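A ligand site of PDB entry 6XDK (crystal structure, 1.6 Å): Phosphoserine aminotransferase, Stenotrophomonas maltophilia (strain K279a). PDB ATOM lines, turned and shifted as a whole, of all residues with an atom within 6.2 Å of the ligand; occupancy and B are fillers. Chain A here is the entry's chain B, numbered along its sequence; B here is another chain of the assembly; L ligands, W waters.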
ATOM      1  N   ALA A  17      10.918  14.881 -15.035  1.00  0.00           N
ATOM      2  CA  ALA A  17      11.755  14.144 -14.091  1.00  0.00           C
ATOM      3  C   ALA A  17      11.026  12.960 -13.472  1.00  0.00           C
ATOM      4  O   ALA A  17      11.666  12.111 -12.846  1.00  0.00           O
ATOM      5  CB  ALA A  17      12.226  15.069 -12.974  1.00  0.00           C
ATOM      6  N   GLY A  82       5.572   0.016  -3.231  1.00  0.00           N
ATOM      7  CA  GLY A  82       5.862   0.989  -2.181  1.00  0.00           C
ATOM      8  C   GLY A  82       6.970   1.992  -2.482  1.00  0.00           C
ATOM      9  O   GLY A  82       7.266   2.846  -1.638  1.00  0.00           O
ATOM     10  N   GLY A  83       7.585   1.920  -3.645  1.00  0.00           N
ATOM     11  CA  GLY A  83       8.541   2.948  -4.018  1.00  0.00           C
ATOM     12  C   GLY A  83       9.873   2.888  -3.296  1.00  0.00           C
ATOM     13  O   GLY A  83      10.177   2.000  -2.488  1.00  0.00           O
ATOM     14  N   ALA A  84      10.710   3.859  -3.644  1.00  0.00           N
ATOM     15  CA  ALA A  84      12.014   3.924  -3.001  1.00  0.00           C
ATOM     16  C   ALA A  84      11.877   4.248  -1.513  1.00  0.00           C
ATOM     17  O   ALA A  84      12.655   3.745  -0.702  1.00  0.00           O
ATOM     18  CB  ALA A  84      12.898   4.956  -3.695  1.00  0.00           C
ATOM     19  N   THR A  85      10.919   5.092  -1.144  1.00  0.00           N
ATOM     20  CA  THR A  85      10.839   5.541   0.254  1.00  0.00           C
ATOM     21  C   THR A  85      10.521   4.375   1.186  1.00  0.00           C
ATOM     22  O   THR A  85      11.051   4.300   2.302  1.00  0.00           O
ATOM     23  CB  THR A  85       9.838   6.682   0.414  1.00  0.00           C
ATOM     24  OG1 THR A  85      10.134   7.723  -0.540  1.00  0.00           O
ATOM     25  CG2 THR A  85       9.973   7.276   1.798  1.00  0.00           C
ATOM     26  N   THR A  86       9.650   3.446   0.753  1.00  0.00           N
ATOM     27  CA  THR A  86       9.435   2.251   1.558  1.00  0.00           C
ATOM     28  C   THR A  86      10.734   1.480   1.772  1.00  0.00           C
ATOM     29  O   THR A  86      11.020   1.041   2.893  1.00  0.00           O
ATOM     30  CB  THR A  86       8.365   1.355   0.914  1.00  0.00           C
ATOM     31  OG1 THR A  86       7.106   2.042   0.924  1.00  0.00           O
ATOM     32  CG2 THR A  86       8.207   0.046   1.736  1.00  0.00           C
ATOM     33  N   GLN A  88      13.668   2.669   1.848  1.00  0.00           N
ATOM     34  CA  GLN A  88      14.519   3.467   2.729  1.00  0.00           C
ATOM     35  C   GLN A  88      14.205   3.228   4.198  1.00  0.00           C
ATOM     36  O   GLN A  88      15.099   3.393   5.047  1.00  0.00           O
ATOM     37  CB  GLN A  88      14.371   4.963   2.383  1.00  0.00           C
ATOM     38  CG  GLN A  88      15.098   5.229   1.057  1.00  0.00           C
ATOM     39  CD  GLN A  88      14.738   6.530   0.412  1.00  0.00           C
ATOM     40  OE1 GLN A  88      13.836   7.227   0.834  1.00  0.00           O
ATOM     41  NE2 GLN A  88      15.436   6.844  -0.685  1.00  0.00           N
ATOM     42  N   TRP A 110      16.910  13.594  -2.129  1.00  0.00           N
ATOM     43  CA  TRP A 110      16.506  12.198  -1.960  1.00  0.00           C
ATOM     44  C   TRP A 110      17.343  11.498  -0.909  1.00  0.00           C
ATOM     45  O   TRP A 110      16.834  10.595  -0.222  1.00  0.00           O
ATOM     46  CB  TRP A 110      16.523  11.475  -3.329  1.00  0.00           C
ATOM     47  CG  TRP A 110      15.483  12.051  -4.228  1.00  0.00           C
ATOM     48  CD1 TRP A 110      15.677  12.781  -5.373  1.00  0.00           C
ATOM     49  CD2 TRP A 110      14.064  12.018  -4.014  1.00  0.00           C
ATOM     50  NE1 TRP A 110      14.467  13.193  -5.883  1.00  0.00           N
ATOM     51  CE2 TRP A 110      13.465  12.728  -5.061  1.00  0.00           C
ATOM     52  CE3 TRP A 110      13.250  11.432  -3.026  1.00  0.00           C
ATOM     53  CZ2 TRP A 110      12.065  12.884  -5.174  1.00  0.00           C
ATOM     54  CZ3 TRP A 110      11.858  11.577  -3.144  1.00  0.00           C
ATOM     55  CH2 TRP A 110      11.289  12.297  -4.209  1.00  0.00           C
ATOM     56  N   THR A 156      23.226   8.336  -2.619  1.00  0.00           N
ATOM     57  CA  THR A 156      22.229   8.551  -3.671  1.00  0.00           C
ATOM     58  C   THR A 156      23.010   8.778  -4.945  1.00  0.00           C
ATOM     59  O   THR A 156      23.716   9.785  -5.076  1.00  0.00           O
ATOM     60  CB  THR A 156      21.340   9.747  -3.348  1.00  0.00           C
ATOM     61  OG1 THR A 156      20.822   9.600  -2.004  1.00  0.00           O
ATOM     62  CG2 THR A 156      20.149   9.856  -4.387  1.00  0.00           C
ATOM     63  N   ASN A 158      22.384   9.446  -8.071  1.00  0.00           N
ATOM     64  CA  ASN A 158      22.058  10.609  -8.874  1.00  0.00           C
ATOM     65  C   ASN A 158      20.963  11.346  -8.152  1.00  0.00           C
ATOM     66  O   ASN A 158      19.909  10.765  -7.875  1.00  0.00           O
ATOM     67  CB  ASN A 158      21.646  10.213 -10.301  1.00  0.00           C
ATOM     68  CG  ASN A 158      21.302  11.418 -11.125  1.00  0.00           C
ATOM     69  OD1 ASN A 158      22.186  12.165 -11.493  1.00  0.00           O
ATOM     70  ND2 ASN A 158      20.015  11.634 -11.411  1.00  0.00           N
ATOM     71  N   GLU A 159      21.231  12.604  -7.791  1.00  0.00           N
ATOM     72  CA  GLU A 159      20.252  13.435  -7.099  1.00  0.00           C
ATOM     73  C   GLU A 159      19.430  14.200  -8.128  1.00  0.00           C
ATOM     74  O   GLU A 159      19.918  15.137  -8.755  1.00  0.00           O
ATOM     75  CB  GLU A 159      20.940  14.362  -6.102  1.00  0.00           C
ATOM     76  CG  GLU A 159      21.178  13.687  -4.743  1.00  0.00           C
ATOM     77  CD  GLU A 159      19.928  13.502  -3.934  1.00  0.00           C
ATOM     78  OE1 GLU A 159      18.817  13.916  -4.353  1.00  0.00           O
ATOM     79  OE2 GLU A 159      20.062  13.020  -2.792  1.00  0.00           O
ATOM     80  N   THR A 160      18.154  13.802  -8.217  1.00  0.00           N
ATOM     81  CA  THR A 160      17.296  14.078  -9.357  1.00  0.00           C
ATOM     82  C   THR A 160      16.847  15.541  -9.392  1.00  0.00           C
ATOM     83  O   THR A 160      16.604  16.093 -10.469  1.00  0.00           O
ATOM     84  CB  THR A 160      16.114  13.085  -9.269  1.00  0.00           C
ATOM     85  OG1 THR A 160      16.619  11.798  -8.846  1.00  0.00           O
ATOM     86  CG2 THR A 160      15.384  12.934 -10.591  1.00  0.00           C
ATOM     87  N   ASP A 180      20.933   4.428  -3.778  1.00  0.00           N
ATOM     88  CA  ASP A 180      19.677   4.760  -4.458  1.00  0.00           C
ATOM     89  C   ASP A 180      19.993   5.170  -5.896  1.00  0.00           C
ATOM     90  O   ASP A 180      20.541   6.258  -6.136  1.00  0.00           O
ATOM     91  CB  ASP A 180      19.002   5.875  -3.679  1.00  0.00           C
ATOM     92  CG  ASP A 180      17.673   6.314  -4.276  1.00  0.00           C
ATOM     93  OD1 ASP A 180      17.278   5.870  -5.368  1.00  0.00           O
ATOM     94  OD2 ASP A 180      17.012   7.145  -3.622  1.00  0.00           O
ATOM     95  N   PHE A 181      19.676   4.292  -6.847  1.00  0.00           N
ATOM     96  CA  PHE A 181      19.864   4.485  -8.287  1.00  0.00           C
ATOM     97  C   PHE A 181      18.535   4.783  -9.005  1.00  0.00           C
ATOM     98  O   PHE A 181      18.447   4.558 -10.216  1.00  0.00           O
ATOM     99  CB  PHE A 181      20.508   3.247  -8.914  1.00  0.00           C
ATOM    100  CG  PHE A 181      22.024   3.269  -8.942  1.00  0.00           C
ATOM    101  CD1 PHE A 181      22.683   3.758 -10.043  1.00  0.00           C
ATOM    102  CD2 PHE A 181      22.755   2.718  -7.902  1.00  0.00           C
ATOM    103  CE1 PHE A 181      24.083   3.737 -10.095  1.00  0.00           C
ATOM    104  CE2 PHE A 181      24.155   2.697  -7.954  1.00  0.00           C
ATOM    105  CZ  PHE A 181      24.799   3.225  -9.042  1.00  0.00           C
ATOM    106  N   SER A 182      17.536   5.297  -8.290  1.00  0.00           N
ATOM    107  CA  SER A 182      16.223   5.522  -8.897  1.00  0.00           C
ATOM    108  C   SER A 182      16.327   6.252 -10.232  1.00  0.00           C
ATOM    109  O   SER A 182      15.721   5.832 -11.213  1.00  0.00           O
ATOM    110  CB  SER A 182      15.303   6.313  -7.951  1.00  0.00           C
ATOM    111  OG  SER A 182      15.040   5.507  -6.805  1.00  0.00           O
ATOM    112  N   SER A 183      17.118   7.313 -10.307  1.00  0.00           N
ATOM    113  CA  SER A 183      17.093   8.108 -11.537  1.00  0.00           C
ATOM    114  C   SER A 183      18.245   7.837 -12.487  1.00  0.00           C
ATOM    115  O   SER A 183      18.312   8.471 -13.549  1.00  0.00           O
ATOM    116  CB  SER A 183      17.048   9.600 -11.186  1.00  0.00           C
ATOM    117  OG  SER A 183      18.043   9.885 -10.215  1.00  0.00           O
ATOM    118  N   TYR A 199      19.116  -0.042  -5.306  1.00  0.00           N
ATOM    119  CA  TYR A 199      17.659  -0.031  -5.409  1.00  0.00           C
ATOM    120  C   TYR A 199      17.196   1.150  -6.244  1.00  0.00           C
ATOM    121  O   TYR A 199      17.929   2.116  -6.452  1.00  0.00           O
ATOM    122  CB  TYR A 199      16.973  -0.024  -4.017  1.00  0.00           C
ATOM    123  CG  TYR A 199      17.157   1.228  -3.175  1.00  0.00           C
ATOM    124  CD1 TYR A 199      18.317   1.430  -2.448  1.00  0.00           C
ATOM    125  CD2 TYR A 199      16.157   2.191  -3.131  1.00  0.00           C
ATOM    126  CE1 TYR A 199      18.476   2.595  -1.677  1.00  0.00           C
ATOM    127  CE2 TYR A 199      16.302   3.340  -2.391  1.00  0.00           C
ATOM    128  CZ  TYR A 199      17.462   3.542  -1.664  1.00  0.00           C
ATOM    129  OH  TYR A 199      17.537   4.686  -0.919  1.00  0.00           O
ATOM    130  N   GLY A 201      13.370   3.287  -7.150  1.00  0.00           N
ATOM    131  CA  GLY A 201      11.926   3.488  -7.227  1.00  0.00           C
ATOM    132  C   GLY A 201      11.427   3.441  -8.652  1.00  0.00           C
ATOM    133  O   GLY A 201      12.205   3.404  -9.608  1.00  0.00           O
ATOM    134  N   ALA A 202      10.090   3.472  -8.775  1.00  0.00           N
ATOM    135  CA  ALA A 202       9.357   3.466 -10.034  1.00  0.00           C
ATOM    136  C   ALA A 202       9.279   4.855 -10.641  1.00  0.00           C
ATOM    137  O   ALA A 202       9.505   5.871  -9.970  1.00  0.00           O
ATOM    138  CB  ALA A 202       7.935   2.954  -9.816  1.00  0.00           C
ATOM    139  N   LYS A 204      11.002   6.443 -12.726  1.00  0.00           N
ATOM    140  CA  LYS A 204      12.222   7.186 -13.047  1.00  0.00           C
ATOM    141  C   LYS A 204      12.926   6.436 -14.190  1.00  0.00           C
ATOM    142  O   LYS A 204      12.293   6.156 -15.201  1.00  0.00           O
ATOM    143  CB  LYS A 204      13.095   7.358 -11.818  1.00  0.00           C
ATOM    144  CG  LYS A 204      12.411   8.149 -10.698  1.00  0.00           C
ATOM    145  CD  LYS A 204      12.241   9.587 -11.115  1.00  0.00           C
ATOM    146  CE  LYS A 204      11.556  10.395 -10.035  1.00  0.00           C
ATOM    147  NZ  LYS A 204      12.474  10.639  -8.901  1.00  0.00           N
ATOM    148  N   TYR A 346      16.207  10.815 -19.448  1.00  0.00           N
ATOM    149  CA  TYR A 346      16.213   9.399 -19.095  1.00  0.00           C
ATOM    150  C   TYR A 346      16.457   8.533 -20.335  1.00  0.00           C
ATOM    151  O   TYR A 346      16.484   8.997 -21.472  1.00  0.00           O
ATOM    152  CB  TYR A 346      14.876   9.039 -18.427  1.00  0.00           C
ATOM    153  CG  TYR A 346      14.702   9.706 -17.077  1.00  0.00           C
ATOM    154  CD1 TYR A 346      15.647   9.544 -16.081  1.00  0.00           C
ATOM    155  CD2 TYR A 346      13.582  10.515 -16.824  1.00  0.00           C
ATOM    156  CE1 TYR A 346      15.512  10.152 -14.853  1.00  0.00           C
ATOM    157  CE2 TYR A 346      13.427  11.153 -15.568  1.00  0.00           C
ATOM    158  CZ  TYR A 346      14.392  10.945 -14.605  1.00  0.00           C
ATOM    159  OH  TYR A 346      14.293  11.536 -13.359  1.00  0.00           O
ATOM    160  N   HIS B  49       1.535  12.463 -10.571  1.00  0.00           N
ATOM    161  CA  HIS B  49       0.469  12.388  -9.591  1.00  0.00           C
ATOM    162  C   HIS B  49       0.140  13.769  -8.993  1.00  0.00           C
ATOM    163  O   HIS B  49      -0.990  13.959  -8.549  1.00  0.00           O
ATOM    164  CB  HIS B  49       0.788  11.365  -8.502  1.00  0.00           C
ATOM    165  CG  HIS B  49       2.057  11.621  -7.747  1.00  0.00           C
ATOM    166  ND1 HIS B  49       3.300  11.271  -8.230  1.00  0.00           N
ATOM    167  CD2 HIS B  49       2.264  12.127  -6.508  1.00  0.00           C
ATOM    168  CE1 HIS B  49       4.223  11.587  -7.323  1.00  0.00           C
ATOM    169  NE2 HIS B  49       3.619  12.108  -6.273  1.00  0.00           N
ATOM    170  N   ILE B 231       7.026   7.001   6.205  1.00  0.00           N
ATOM    171  CA  ILE B 231       6.327   6.259   5.142  1.00  0.00           C
ATOM    172  C   ILE B 231       5.402   5.178   5.711  1.00  0.00           C
ATOM    173  O   ILE B 231       4.506   4.675   5.010  1.00  0.00           O
ATOM    174  CB  ILE B 231       7.395   5.676   4.184  1.00  0.00           C
ATOM    175  CG1 ILE B 231       6.747   5.116   2.905  1.00  0.00           C
ATOM    176  CG2 ILE B 231       8.222   4.564   4.877  1.00  0.00           C
ATOM    177  CD1 ILE B 231       6.060   6.216   2.065  1.00  0.00           C
ATOM    178  N   ASN B 245       4.412   9.453  -0.963  1.00  0.00           N
ATOM    179  CA  ASN B 245       5.445   9.263  -1.978  1.00  0.00           C
ATOM    180  C   ASN B 245       4.773   8.960  -3.301  1.00  0.00           C
ATOM    181  O   ASN B 245       3.569   9.201  -3.463  1.00  0.00           O
ATOM    182  CB  ASN B 245       6.455   8.179  -1.548  1.00  0.00           C
ATOM    183  CG  ASN B 245       5.878   6.779  -1.545  1.00  0.00           C
ATOM    184  OD1 ASN B 245       4.686   6.583  -1.305  1.00  0.00           O
ATOM    185  ND2 ASN B 245       6.739   5.781  -1.823  1.00  0.00           N
ATOM    186  N   THR B 246       5.512   8.441  -4.283  1.00  0.00           N
ATOM    187  CA  THR B 246       4.916   8.171  -5.599  1.00  0.00           C
ATOM    188  C   THR B 246       3.868   7.076  -5.478  1.00  0.00           C
ATOM    189  O   THR B 246       4.207   5.951  -5.088  1.00  0.00           O
ATOM    190  CB  THR B 246       5.997   7.757  -6.589  1.00  0.00           C
ATOM    191  OG1 THR B 246       7.036   8.746  -6.624  1.00  0.00           O
ATOM    192  CG2 THR B 246       5.415   7.585  -7.985  1.00  0.00           C
ATOM    193  N   PRO B 247       2.602   7.330  -5.796  1.00  0.00           N
ATOM    194  CA  PRO B 247       1.577   6.306  -5.698  1.00  0.00           C
ATOM    195  C   PRO B 247       1.527   5.490  -6.981  1.00  0.00           C
ATOM    196  O   PRO B 247       2.124   5.880  -7.991  1.00  0.00           O
ATOM    197  CB  PRO B 247       0.288   7.127  -5.518  1.00  0.00           C
ATOM    198  CG  PRO B 247       0.543   8.297  -6.391  1.00  0.00           C
ATOM    199  CD  PRO B 247       2.031   8.625  -6.217  1.00  0.00           C
HETATM  200  N1  LIG L   1      14.858   8.484  -4.949  1.00  0.00           N
HETATM  201  C1  LIG L   1      15.275   9.125  -6.054  1.00  0.00           C
HETATM  202  C2  LIG L   1      16.754   9.245  -6.287  1.00  0.00           C
HETATM  203  C3  LIG L   1      14.351   9.675  -6.955  1.00  0.00           C
HETATM  204  O1  LIG L   1      14.794  10.225  -8.105  1.00  0.00           O
HETATM  205  C4  LIG L   1      12.977   9.563  -6.720  1.00  0.00           C
HETATM  206  C5  LIG L   1      12.007  10.037  -7.692  1.00  0.00           C
HETATM  207  C6  LIG L   1      12.566   8.914  -5.544  1.00  0.00           C
HETATM  208  C7  LIG L   1      13.540   8.396  -4.719  1.00  0.00           C
HETATM  209  C8  LIG L   1      11.107   8.840  -5.190  1.00  0.00           C
HETATM  210  O2  LIG L   1      10.861   8.045  -4.045  1.00  0.00           O
HETATM  211  P1  LIG L   1       9.485   7.148  -4.114  1.00  0.00           P
HETATM  212  O3  LIG L   1       8.421   8.187  -4.529  1.00  0.00           O
HETATM  213  O4  LIG L   1       9.246   6.628  -2.700  1.00  0.00           O
HETATM  214  O5  LIG L   1       9.655   6.096  -5.209  1.00  0.00           O
HETATM  215  O   HOH W   1       8.257  10.504  -3.044  1.00  0.00           O
HETATM  216  O   HOH W   2      11.349   6.713  -7.598  1.00  0.00           O
HETATM  217  O   HOH W   3      12.923   8.501  -1.436  1.00  0.00           O
HETATM  218  O   HOH W   4       8.232   4.805  -6.798  1.00  0.00           O
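The side-chain hydroxyl (OG1) of Thr 85 is in hydrogen-bond range of an oxygen (O4) of the ligand, at 2.6 Å.
ND2 of Asn 245 of chain B is in hydrogen-bond range of O4 of the ligand (2.8 Å).
NZ of Lys 204 is bonded to C5 of the ligand (1.4 Å).
The backbone NH (N) of Thr 85 lies within hydrogen-bond range of an oxygen (O4) of the ligand.
The side-chain carboxylate (OD2) of Asp 180 lies within hydrogen-bond range of a nitrogen (N1) of the ligand (2.9 Å).
N of Ala 84 lies within hydrogen-bond range of O5 of the ligand (2.9 Å).
OG1 of Thr 246 of chain B lies within hydrogen-bond range of O3 of the ligand (2.6 Å).
The side-chain hydroxyl of Thr 160 sits at hydrogen-bond distance from an oxygen (O1) of the ligand (2.5 Å).
O3 of the ligand is in hydrogen-bond range of N of Thr 246 of chain B (2.9 Å).
The side-chain carboxylate (OD2) of Asp 180 sits at hydrogen-bond distance from the side-chain amide nitrogen (NE2) of Gln 88, 3.3 Å away.
ND2 of Asn 245 of chain B lies within hydrogen-bond range of O of Gly 82, at 3.0 Å.
The side-chain carboxylate (OD1) of Asp 180 lies within hydrogen-bond range of the side-chain hydroxyl (OG) of Ser 182.
The side-chain hydroxyl (OG) of Ser 182 is in hydrogen-bond range of the backbone NH (N) of Gly 201, 2.8 Å away.
The side-chain hydroxyl (OG1) of Thr 160 is in hydrogen-bond range of the side-chain hydroxyl (OG) of Ser 183 (2.7 Å).
ND2 of Asn 158 sits at hydrogen-bond distance from OG of Ser 183 (2.9 Å).
N of Trp 110 sits at hydrogen-bond distance from OE1 of Glu 159.
Residues that only touch the ligand: Gly 83 (3.5 Å), Trp 110 (3.5 Å), Thr 156 (3.9 Å), Asn 158 (3.8 Å), Ser 182 (3.4 Å) and Ser 183 (3.9 Å).
Hydrophobic or aromatic side chains that line the ligand: Ala 84 and Trp 110.
Of the 26 residues printed, 13 come within 4 Å of the ligand.
The nearest printed residue that does not touch the ligand is Gly 201 (4.004 Å).
Water W4 bridges O5 of the ligand and N of Ala 202.
Water W2 lies within hydrogen-bond range of an oxygen (O5) of the ligand (3.0 Å) and the backbone carbonyl oxygen (O) of Ala 202 (3.1 Å).
Water W3 lies within hydrogen-bond range of the side-chain amide oxygen (OE1) of Gln 88, the side-chain hydroxyl (OG1) of Thr 85 and an oxygen (O2) of the ligand.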
